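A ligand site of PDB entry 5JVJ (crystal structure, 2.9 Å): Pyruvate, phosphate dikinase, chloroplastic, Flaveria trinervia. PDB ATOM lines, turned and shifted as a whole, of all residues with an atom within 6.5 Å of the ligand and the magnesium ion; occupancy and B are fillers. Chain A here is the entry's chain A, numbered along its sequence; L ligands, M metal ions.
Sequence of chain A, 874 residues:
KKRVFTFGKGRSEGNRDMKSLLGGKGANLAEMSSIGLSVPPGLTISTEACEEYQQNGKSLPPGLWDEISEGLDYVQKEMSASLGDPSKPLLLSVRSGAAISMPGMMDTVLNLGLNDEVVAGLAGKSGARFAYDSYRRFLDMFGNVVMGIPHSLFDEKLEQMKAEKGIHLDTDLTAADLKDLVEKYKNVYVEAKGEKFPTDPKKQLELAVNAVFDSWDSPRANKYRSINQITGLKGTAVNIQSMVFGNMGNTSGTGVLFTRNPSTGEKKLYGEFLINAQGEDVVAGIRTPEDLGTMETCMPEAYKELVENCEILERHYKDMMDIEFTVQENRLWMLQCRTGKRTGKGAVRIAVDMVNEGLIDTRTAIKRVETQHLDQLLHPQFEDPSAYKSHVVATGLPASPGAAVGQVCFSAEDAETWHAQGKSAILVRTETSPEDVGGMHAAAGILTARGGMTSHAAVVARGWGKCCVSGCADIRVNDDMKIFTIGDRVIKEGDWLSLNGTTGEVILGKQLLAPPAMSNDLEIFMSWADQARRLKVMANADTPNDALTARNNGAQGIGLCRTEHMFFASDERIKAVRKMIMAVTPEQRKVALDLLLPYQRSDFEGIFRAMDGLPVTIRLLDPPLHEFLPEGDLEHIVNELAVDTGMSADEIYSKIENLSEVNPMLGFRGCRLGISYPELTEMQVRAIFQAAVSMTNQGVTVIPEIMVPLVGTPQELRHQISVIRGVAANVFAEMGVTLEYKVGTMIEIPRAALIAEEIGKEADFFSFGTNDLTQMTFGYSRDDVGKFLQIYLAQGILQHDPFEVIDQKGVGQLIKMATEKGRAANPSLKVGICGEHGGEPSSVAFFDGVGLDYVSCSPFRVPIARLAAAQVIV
The backbone carbonyl oxygen of Gly 769 lies close to an oxygen (O2) of the ligand (3.2 Å).
Leu 560 touches the ligand (CD2 to C3, 3.7 Å).
Met 746 touches the ligand (CE to C2, 3.9 Å).
Cys 834 touches the ligand (SG to C3, 3.5 Å).
Gly 835 touches the ligand.
Hydrophobic or aromatic side chains that line the ligand: Leu 560 and Met 746.
12 residues have an atom within 4 Å of the ligand: Leu 560, Arg 562, Arg 619, Met 746, Glu 748, Gly 769, Thr 770, Asn 771, Asp 772, Arg 782, Cys 834 and Gly 835.
The nearest printed residue that does not touch the ligand is Arg 669 (4.1 Å).
N of Asp 622 sits at hydrogen-bond distance from OE1 of Glu 564 (3.1 Å).
The backbone carbonyl oxygen (O) of Phe 768 is in hydrogen-bond range of the backbone NH (N) of Gly 835 (3.5 Å).
The side-chain sulfur (SD) of Met 746 lies close to the side-chain sulfur (SG) of Cys 834 (3.6 Å).
The side-chain amide oxygen (OD1) of Asn 771 sits at hydrogen-bond distance from the backbone NH (N) of Glu 836, 3.0 Å away.
O of Phe 768 lies within hydrogen-bond range of N of Cys 834, 3.1 Å away.
The backbone carbonyl oxygen (O) of Cys 834 is in hydrogen-bond range of the side-chain amide nitrogen (ND2) of Asn 540.
The guanidinium group (NH1) of Arg 619 sits close to the side-chain sulfur (SD) of Met 746, 3.8 Å away.
N of Leu 773 sits at hydrogen-bond distance from O of Glu 748 (3.4 Å).
The magnesium ion is bound by OE1 of Glu 748 (2.1 Å), O4 of the ligand (2.1 Å) and OD2 of Asp 772 (2.6 Å).
Slightly farther from the magnesium ion lies O3 of the ligand (2.7 Å).
Slightly farther from the magnesium ion lies an oxygen (O1) of the ligand (2.8 Å).
O6 of the ligand lies within salt-bridge range of NH2 of Arg 619 (3.0 Å).
An oxygen (O1) of the ligand lies within hydrogen-bond range of the backbone NH (N) of Asp 772 (3.3 Å).
An oxygen (O5) of the ligand is in salt-bridge range of the guanidinium group (NH2) of Arg 782 (3.2 Å).
An oxygen (O2) of the ligand is in hydrogen-bond range of the backbone NH (N) of Thr 770 (3.3 Å).
The guanidinium group (NE) of Arg 562 lies within salt-bridge range of an oxygen (O6) of the ligand, 3.0 Å away.
An oxygen (O2) of the ligand is in hydrogen-bond range of the backbone NH (N) of Asn 771.
ND2 of Asn 771 lies within hydrogen-bond range of O5 of the ligand, at 3.1 Å.
Arg 619 touches the magnesium ion.
Asp 622 touches the magnesium ion.
Four residues have an atom within 4 Å of the magnesium ion: Arg 619, Asp 622, Glu 748 and Asp 772.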
ATOM      1  N   ASN A 540       9.821 -10.102 -21.643  1.00  0.00           N
ATOM      2  CA  ASN A 540       9.393  -9.225 -22.734  1.00  0.00           C
ATOM      3  C   ASN A 540      10.224  -7.945 -22.648  1.00  0.00           C
ATOM      4  O   ASN A 540       9.963  -7.074 -21.812  1.00  0.00           O
ATOM      5  CB  ASN A 540       7.910  -8.931 -22.637  1.00  0.00           C
ATOM      6  CG  ASN A 540       7.050 -10.179 -22.708  1.00  0.00           C
ATOM      7  OD1 ASN A 540       7.507 -11.235 -23.139  1.00  0.00           O
ATOM      8  ND2 ASN A 540       5.806 -10.063 -22.275  1.00  0.00           N
ATOM      9  N   LEU A 560       9.716 -12.392 -25.979  1.00  0.00           N
ATOM     10  CA  LEU A 560       9.111 -11.454 -26.917  1.00  0.00           C
ATOM     11  C   LEU A 560       9.919 -10.168 -26.932  1.00  0.00           C
ATOM     12  O   LEU A 560       9.969  -9.463 -25.919  1.00  0.00           O
ATOM     13  CB  LEU A 560       7.659 -11.179 -26.532  1.00  0.00           C
ATOM     14  CG  LEU A 560       6.985 -10.059 -27.342  1.00  0.00           C
ATOM     15  CD1 LEU A 560       6.912 -10.438 -28.817  1.00  0.00           C
ATOM     16  CD2 LEU A 560       5.595  -9.752 -26.797  1.00  0.00           C
ATOM     17  N   ARG A 562       9.516  -6.836 -28.951  1.00  0.00           N
ATOM     18  CA  ARG A 562       8.582  -6.138 -29.828  1.00  0.00           C
ATOM     19  C   ARG A 562       9.352  -5.142 -30.685  1.00  0.00           C
ATOM     20  O   ARG A 562       9.749  -4.076 -30.221  1.00  0.00           O
ATOM     21  CB  ARG A 562       7.508  -5.427 -29.004  1.00  0.00           C
ATOM     22  CG  ARG A 562       6.500  -6.343 -28.318  1.00  0.00           C
ATOM     23  CD  ARG A 562       5.557  -5.495 -27.456  1.00  0.00           C
ATOM     24  NE  ARG A 562       4.382  -6.229 -26.993  1.00  0.00           N
ATOM     25  CZ  ARG A 562       4.253  -6.819 -25.807  1.00  0.00           C
ATOM     26  NH1 ARG A 562       5.254  -6.793 -24.927  1.00  0.00           N
ATOM     27  NH2 ARG A 562       3.133  -7.442 -25.492  1.00  0.00           N
ATOM     28  N   GLU A 564       8.392  -3.185 -33.043  1.00  0.00           N
ATOM     29  CA  GLU A 564       7.727  -1.895 -33.203  1.00  0.00           C
ATOM     30  C   GLU A 564       8.039  -0.936 -32.049  1.00  0.00           C
ATOM     31  O   GLU A 564       7.830   0.270 -32.195  1.00  0.00           O
ATOM     32  CB  GLU A 564       6.210  -2.074 -33.313  1.00  0.00           C
ATOM     33  CG  GLU A 564       5.544  -2.738 -32.120  1.00  0.00           C
ATOM     34  CD  GLU A 564       5.535  -4.253 -32.187  1.00  0.00           C
ATOM     35  OE1 GLU A 564       6.284  -4.824 -33.022  1.00  0.00           O
ATOM     36  OE2 GLU A 564       4.782  -4.862 -31.410  1.00  0.00           O
ATOM     37  N   HIS A 565       8.516  -1.446 -30.922  1.00  0.00           N
ATOM     38  CA  HIS A 565       8.826  -0.630 -29.753  1.00  0.00           C
ATOM     39  C   HIS A 565      10.308  -0.282 -29.671  1.00  0.00           C
ATOM     40  O   HIS A 565      10.795   0.046 -28.581  1.00  0.00           O
ATOM     41  CB  HIS A 565       8.380  -1.344 -28.472  1.00  0.00           C
ATOM     42  CG  HIS A 565       6.893  -1.338 -28.251  1.00  0.00           C
ATOM     43  ND1 HIS A 565       6.039  -0.532 -28.962  1.00  0.00           N
ATOM     44  CD2 HIS A 565       6.125  -2.032 -27.381  1.00  0.00           C
ATOM     45  CE1 HIS A 565       4.799  -0.732 -28.544  1.00  0.00           C
ATOM     46  NE2 HIS A 565       4.827  -1.645 -27.588  1.00  0.00           N
ATOM     47  N   ARG A 619      10.289 -10.683 -32.647  1.00  0.00           N
ATOM     48  CA  ARG A 619       9.042 -10.723 -33.393  1.00  0.00           C
ATOM     49  C   ARG A 619       9.063  -9.677 -34.500  1.00  0.00           C
ATOM     50  O   ARG A 619       9.557  -8.557 -34.299  1.00  0.00           O
ATOM     51  CB  ARG A 619       7.840 -10.475 -32.468  1.00  0.00           C
ATOM     52  CG  ARG A 619       6.507 -10.698 -33.140  1.00  0.00           C
ATOM     53  CD  ARG A 619       5.358 -10.586 -32.153  1.00  0.00           C
ATOM     54  NE  ARG A 619       4.988  -9.200 -31.882  1.00  0.00           N
ATOM     55  CZ  ARG A 619       4.053  -8.834 -31.017  1.00  0.00           C
ATOM     56  NH1 ARG A 619       3.382  -9.751 -30.327  1.00  0.00           N
ATOM     57  NH2 ARG A 619       3.784  -7.553 -30.830  1.00  0.00           N
ATOM     58  N   ASP A 622       4.880  -5.257 -35.806  1.00  0.00           N
ATOM     59  CA  ASP A 622       3.419  -5.214 -35.642  1.00  0.00           C
ATOM     60  C   ASP A 622       3.052  -3.818 -35.145  1.00  0.00           C
ATOM     61  O   ASP A 622       2.681  -3.627 -33.989  1.00  0.00           O
ATOM     62  CB  ASP A 622       2.939  -6.290 -34.673  1.00  0.00           C
ATOM     63  CG  ASP A 622       1.452  -6.209 -34.388  1.00  0.00           C
ATOM     64  OD1 ASP A 622       0.728  -5.620 -35.232  1.00  0.00           O
ATOM     65  OD2 ASP A 622       1.001  -6.736 -33.355  1.00  0.00           O
ATOM     66  N   MET A 665      -6.909  -1.880 -34.662  1.00  0.00           N
ATOM     67  CA  MET A 665      -6.523  -3.103 -33.953  1.00  0.00           C
ATOM     68  C   MET A 665      -6.793  -4.347 -34.790  1.00  0.00           C
ATOM     69  O   MET A 665      -6.161  -5.381 -34.559  1.00  0.00           O
ATOM     70  CB  MET A 665      -7.259  -3.202 -32.624  1.00  0.00           C
ATOM     71  CG  MET A 665      -6.437  -3.897 -31.542  1.00  0.00           C
ATOM     72  SD  MET A 665      -5.045  -2.895 -30.986  1.00  0.00           S
ATOM     73  CE  MET A 665      -3.848  -4.162 -30.593  1.00  0.00           C
ATOM     74  N   ARG A 669      -1.998  -4.464 -40.005  1.00  0.00           N
ATOM     75  CA  ARG A 669      -0.911  -4.594 -39.043  1.00  0.00           C
ATOM     76  C   ARG A 669      -0.544  -6.077 -38.922  1.00  0.00           C
ATOM     77  O   ARG A 669      -1.098  -6.934 -39.603  1.00  0.00           O
ATOM     78  CB  ARG A 669      -1.300  -4.007 -37.685  1.00  0.00           C
ATOM     79  CG  ARG A 669      -2.502  -4.677 -37.021  1.00  0.00           C
ATOM     80  CD  ARG A 669      -2.108  -5.217 -35.651  1.00  0.00           C
ATOM     81  NE  ARG A 669      -3.239  -5.665 -34.865  1.00  0.00           N
ATOM     82  CZ  ARG A 669      -3.139  -6.250 -33.673  1.00  0.00           C
ATOM     83  NH1 ARG A 669      -1.949  -6.458 -33.132  1.00  0.00           N
ATOM     84  NH2 ARG A 669      -4.235  -6.613 -33.020  1.00  0.00           N
ATOM     85  N   PRO A 709       3.786 -12.224 -36.159  1.00  0.00           N
ATOM     86  CA  PRO A 709       2.628 -11.778 -35.373  1.00  0.00           C
ATOM     87  C   PRO A 709       1.297 -11.905 -36.100  1.00  0.00           C
ATOM     88  O   PRO A 709       1.248 -11.861 -37.333  1.00  0.00           O
ATOM     89  CB  PRO A 709       2.973 -10.313 -35.097  1.00  0.00           C
ATOM     90  CG  PRO A 709       3.670  -9.884 -36.348  1.00  0.00           C
ATOM     91  CD  PRO A 709       4.428 -11.106 -36.865  1.00  0.00           C
ATOM     92  N   LEU A 710       0.222 -12.029 -35.329  1.00  0.00           N
ATOM     93  CA  LEU A 710      -1.148 -11.898 -35.828  1.00  0.00           C
ATOM     94  C   LEU A 710      -1.427 -12.887 -36.955  1.00  0.00           C
ATOM     95  O   LEU A 710      -2.020 -12.546 -37.983  1.00  0.00           O
ATOM     96  CB  LEU A 710      -1.428 -10.455 -36.269  1.00  0.00           C
ATOM     97  CG  LEU A 710      -2.832  -9.916 -35.937  1.00  0.00           C
ATOM     98  CD1 LEU A 710      -3.026  -9.807 -34.435  1.00  0.00           C
ATOM     99  CD2 LEU A 710      -3.050  -8.564 -36.606  1.00  0.00           C
ATOM    100  N   MET A 746       3.114 -16.142 -33.222  1.00  0.00           N
ATOM    101  CA  MET A 746       2.125 -15.792 -32.209  1.00  0.00           C
ATOM    102  C   MET A 746       0.848 -16.594 -32.451  1.00  0.00           C
ATOM    103  O   MET A 746       0.440 -16.817 -33.588  1.00  0.00           O
ATOM    104  CB  MET A 746       1.817 -14.292 -32.272  1.00  0.00           C
ATOM    105  CG  MET A 746       2.956 -13.392 -31.819  1.00  0.00           C
ATOM    106  SD  MET A 746       3.322 -13.510 -30.052  1.00  0.00           S
ATOM    107  CE  MET A 746       1.779 -12.940 -29.336  1.00  0.00           C
ATOM    108  N   GLU A 748      -2.368 -15.441 -31.385  1.00  0.00           N
ATOM    109  CA  GLU A 748      -3.178 -14.368 -30.818  1.00  0.00           C
ATOM    110  C   GLU A 748      -4.434 -14.100 -31.655  1.00  0.00           C
ATOM    111  O   GLU A 748      -5.091 -13.081 -31.436  1.00  0.00           O
ATOM    112  CB  GLU A 748      -2.349 -13.085 -30.708  1.00  0.00           C
ATOM    113  CG  GLU A 748      -1.686 -12.655 -32.010  1.00  0.00           C
ATOM    114  CD  GLU A 748      -0.852 -11.395 -31.843  1.00  0.00           C
ATOM    115  OE1 GLU A 748      -0.858 -10.816 -30.741  1.00  0.00           O
ATOM    116  OE2 GLU A 748      -0.204 -10.984 -32.834  1.00  0.00           O
ATOM    117  N   PHE A 768       1.371 -17.696 -27.144  1.00  0.00           N
ATOM    118  CA  PHE A 768       0.024 -17.149 -27.033  1.00  0.00           C
ATOM    119  C   PHE A 768       0.096 -15.659 -26.692  1.00  0.00           C
ATOM    120  O   PHE A 768       0.712 -15.274 -25.694  1.00  0.00           O
ATOM    121  CB  PHE A 768      -0.778 -17.905 -25.975  1.00  0.00           C
ATOM    122  CG  PHE A 768      -1.060 -19.327 -26.341  1.00  0.00           C
ATOM    123  CD1 PHE A 768      -2.059 -19.635 -27.257  1.00  0.00           C
ATOM    124  CD2 PHE A 768      -0.348 -20.359 -25.772  1.00  0.00           C
ATOM    125  CE1 PHE A 768      -2.325 -20.937 -27.600  1.00  0.00           C
ATOM    126  CE2 PHE A 768      -0.605 -21.666 -26.105  1.00  0.00           C
ATOM    127  CZ  PHE A 768      -1.596 -21.963 -27.023  1.00  0.00           C
ATOM    128  N   GLY A 769      -0.523 -14.823 -27.527  1.00  0.00           N
ATOM    129  CA  GLY A 769      -0.685 -13.423 -27.214  1.00  0.00           C
ATOM    130  C   GLY A 769      -2.057 -13.141 -26.616  1.00  0.00           C
ATOM    131  O   GLY A 769      -2.966 -12.711 -27.321  1.00  0.00           O
ATOM    132  N   THR A 770      -2.206 -13.377 -25.313  1.00  0.00           N
ATOM    133  CA  THR A 770      -3.519 -13.323 -24.690  1.00  0.00           C
ATOM    134  C   THR A 770      -4.095 -11.916 -24.613  1.00  0.00           C
ATOM    135  O   THR A 770      -5.266 -11.777 -24.225  1.00  0.00           O
ATOM    136  CB  THR A 770      -3.452 -13.934 -23.290  1.00  0.00           C
ATOM    137  OG1 THR A 770      -2.336 -13.374 -22.586  1.00  0.00           O
ATOM    138  CG2 THR A 770      -3.295 -15.437 -23.371  1.00  0.00           C
ATOM    139  N   ASN A 771      -3.333 -10.891 -24.967  1.00  0.00           N
ATOM    140  CA  ASN A 771      -3.906  -9.547 -25.067  1.00  0.00           C
ATOM    141  C   ASN A 771      -4.827  -9.453 -26.272  1.00  0.00           C
ATOM    142  O   ASN A 771      -5.995  -9.065 -26.148  1.00  0.00           O
ATOM    143  CB  ASN A 771      -2.785  -8.504 -25.141  1.00  0.00           C
ATOM    144  CG  ASN A 771      -1.790  -8.639 -24.009  1.00  0.00           C
ATOM    145  OD1 ASN A 771      -2.095  -9.206 -22.960  1.00  0.00           O
ATOM    146  ND2 ASN A 771      -0.591  -8.103 -24.206  1.00  0.00           N
ATOM    147  N   ASP A 772      -4.308  -9.794 -27.454  1.00  0.00           N
ATOM    148  CA  ASP A 772      -5.147  -9.782 -28.649  1.00  0.00           C
ATOM    149  C   ASP A 772      -6.145 -10.935 -28.628  1.00  0.00           C
ATOM    150  O   ASP A 772      -7.318 -10.753 -28.967  1.00  0.00           O
ATOM    151  CB  ASP A 772      -4.272  -9.876 -29.903  1.00  0.00           C
ATOM    152  CG  ASP A 772      -3.639  -8.546 -30.267  1.00  0.00           C
ATOM    153  OD1 ASP A 772      -4.376  -7.547 -30.375  1.00  0.00           O
ATOM    154  OD2 ASP A 772      -2.400  -8.503 -30.445  1.00  0.00           O
ATOM    155  N   LEU A 773      -5.701 -12.122 -28.209  1.00  0.00           N
ATOM    156  CA  LEU A 773      -6.601 -13.273 -28.175  1.00  0.00           C
ATOM    157  C   LEU A 773      -7.809 -12.982 -27.293  1.00  0.00           C
ATOM    158  O   LEU A 773      -8.954 -13.223 -27.690  1.00  0.00           O
ATOM    159  CB  LEU A 773      -5.842 -14.508 -27.671  1.00  0.00           C
ATOM    160  CG  LEU A 773      -6.616 -15.832 -27.720  1.00  0.00           C
ATOM    161  CD1 LEU A 773      -7.045 -16.174 -29.139  1.00  0.00           C
ATOM    162  CD2 LEU A 773      -5.776 -16.952 -27.133  1.00  0.00           C
ATOM    163  N   ARG A 782      -9.381  -3.466 -26.333  1.00  0.00           N
ATOM    164  CA  ARG A 782      -8.503  -3.291 -25.166  1.00  0.00           C
ATOM    165  C   ARG A 782      -8.354  -1.826 -24.796  1.00  0.00           C
ATOM    166  O   ARG A 782      -8.153  -1.497 -23.622  1.00  0.00           O
ATOM    167  CB  ARG A 782      -7.145  -3.942 -25.464  1.00  0.00           C
ATOM    168  CG  ARG A 782      -6.466  -3.441 -26.730  1.00  0.00           C
ATOM    169  CD  ARG A 782      -5.414  -4.426 -27.234  1.00  0.00           C
ATOM    170  NE  ARG A 782      -4.228  -4.515 -26.388  1.00  0.00           N
ATOM    171  CZ  ARG A 782      -3.150  -5.248 -26.698  1.00  0.00           C
ATOM    172  NH1 ARG A 782      -3.112  -5.940 -27.833  1.00  0.00           N
ATOM    173  NH2 ARG A 782      -2.112  -5.272 -25.884  1.00  0.00           N
ATOM    174  N   ILE A 833       3.712 -18.207 -23.499  1.00  0.00           N
ATOM    175  CA  ILE A 833       2.704 -17.158 -23.351  1.00  0.00           C
ATOM    176  C   ILE A 833       3.435 -15.857 -23.050  1.00  0.00           C
ATOM    177  O   ILE A 833       4.136 -15.748 -22.048  1.00  0.00           O
ATOM    178  CB  ILE A 833       1.689 -17.525 -22.236  1.00  0.00           C
ATOM    179  CG1 ILE A 833       0.960 -16.287 -21.695  1.00  0.00           C
ATOM    180  CG2 ILE A 833       2.384 -18.238 -21.096  1.00  0.00           C
ATOM    181  CD1 ILE A 833       0.015 -15.669 -22.682  1.00  0.00           C
ATOM    182  N   CYS A 834       3.267 -14.863 -23.921  1.00  0.00           N
ATOM    183  CA  CYS A 834       3.890 -13.558 -23.737  1.00  0.00           C
ATOM    184  C   CYS A 834       2.887 -12.435 -23.508  1.00  0.00           C
ATOM    185  O   CYS A 834       3.291 -11.278 -23.390  1.00  0.00           O
ATOM    186  CB  CYS A 834       4.766 -13.207 -24.940  1.00  0.00           C
ATOM    187  SG  CYS A 834       3.853 -13.153 -26.494  1.00  0.00           S
ATOM    188  N   GLY A 835       1.599 -12.742 -23.466  1.00  0.00           N
ATOM    189  CA  GLY A 835       0.617 -11.747 -23.067  1.00  0.00           C
ATOM    190  C   GLY A 835       0.817 -11.305 -21.635  1.00  0.00           C
ATOM    191  O   GLY A 835       1.570 -11.895 -20.851  1.00  0.00           O
ATOM    192  N   GLU A 836       0.118 -10.227 -21.278  1.00  0.00           N
ATOM    193  CA  GLU A 836       0.283  -9.650 -19.948  1.00  0.00           C
ATOM    194  C   GLU A 836      -0.112 -10.624 -18.845  1.00  0.00           C
ATOM    195  O   GLU A 836       0.336 -10.454 -17.702  1.00  0.00           O
ATOM    196  CB  GLU A 836      -0.519  -8.358 -19.826  1.00  0.00           C
ATOM    197  CG  GLU A 836       0.075  -7.206 -20.626  1.00  0.00           C
ATOM    198  CD  GLU A 836       1.466  -6.817 -20.146  1.00  0.00           C
ATOM    199  OE1 GLU A 836       1.572  -6.304 -19.009  1.00  0.00           O
ATOM    200  OE2 GLU A 836       2.442  -7.036 -20.892  1.00  0.00           O
HETATM  201  C1  LIG L   1      -0.407  -9.951 -27.439  1.00  0.00           C
HETATM  202  O1  LIG L   1      -1.125  -9.618 -28.373  1.00  0.00           O
HETATM  203  O2  LIG L   1      -0.830 -10.573 -26.372  1.00  0.00           O
HETATM  204  C2  LIG L   1       1.060  -9.669 -27.424  1.00  0.00           C
HETATM  205  C3  LIG L   1       1.903 -10.220 -26.586  1.00  0.00           C
HETATM  206  O3  LIG L   1       1.397  -8.755 -28.411  1.00  0.00           O
HETATM  207  P1  LIG L   1       0.810  -7.292 -28.375  1.00  0.00           P
HETATM  208  O4  LIG L   1      -0.304  -7.266 -29.445  1.00  0.00           O
HETATM  209  O5  LIG L   1       0.319  -7.004 -26.995  1.00  0.00           O
HETATM  210  O6  LIG L   1       1.950  -6.367 -28.812  1.00  0.00           O
HETATM  211 MG    MG M   1       0.124  -8.915 -30.750  1.00  0.00          MG
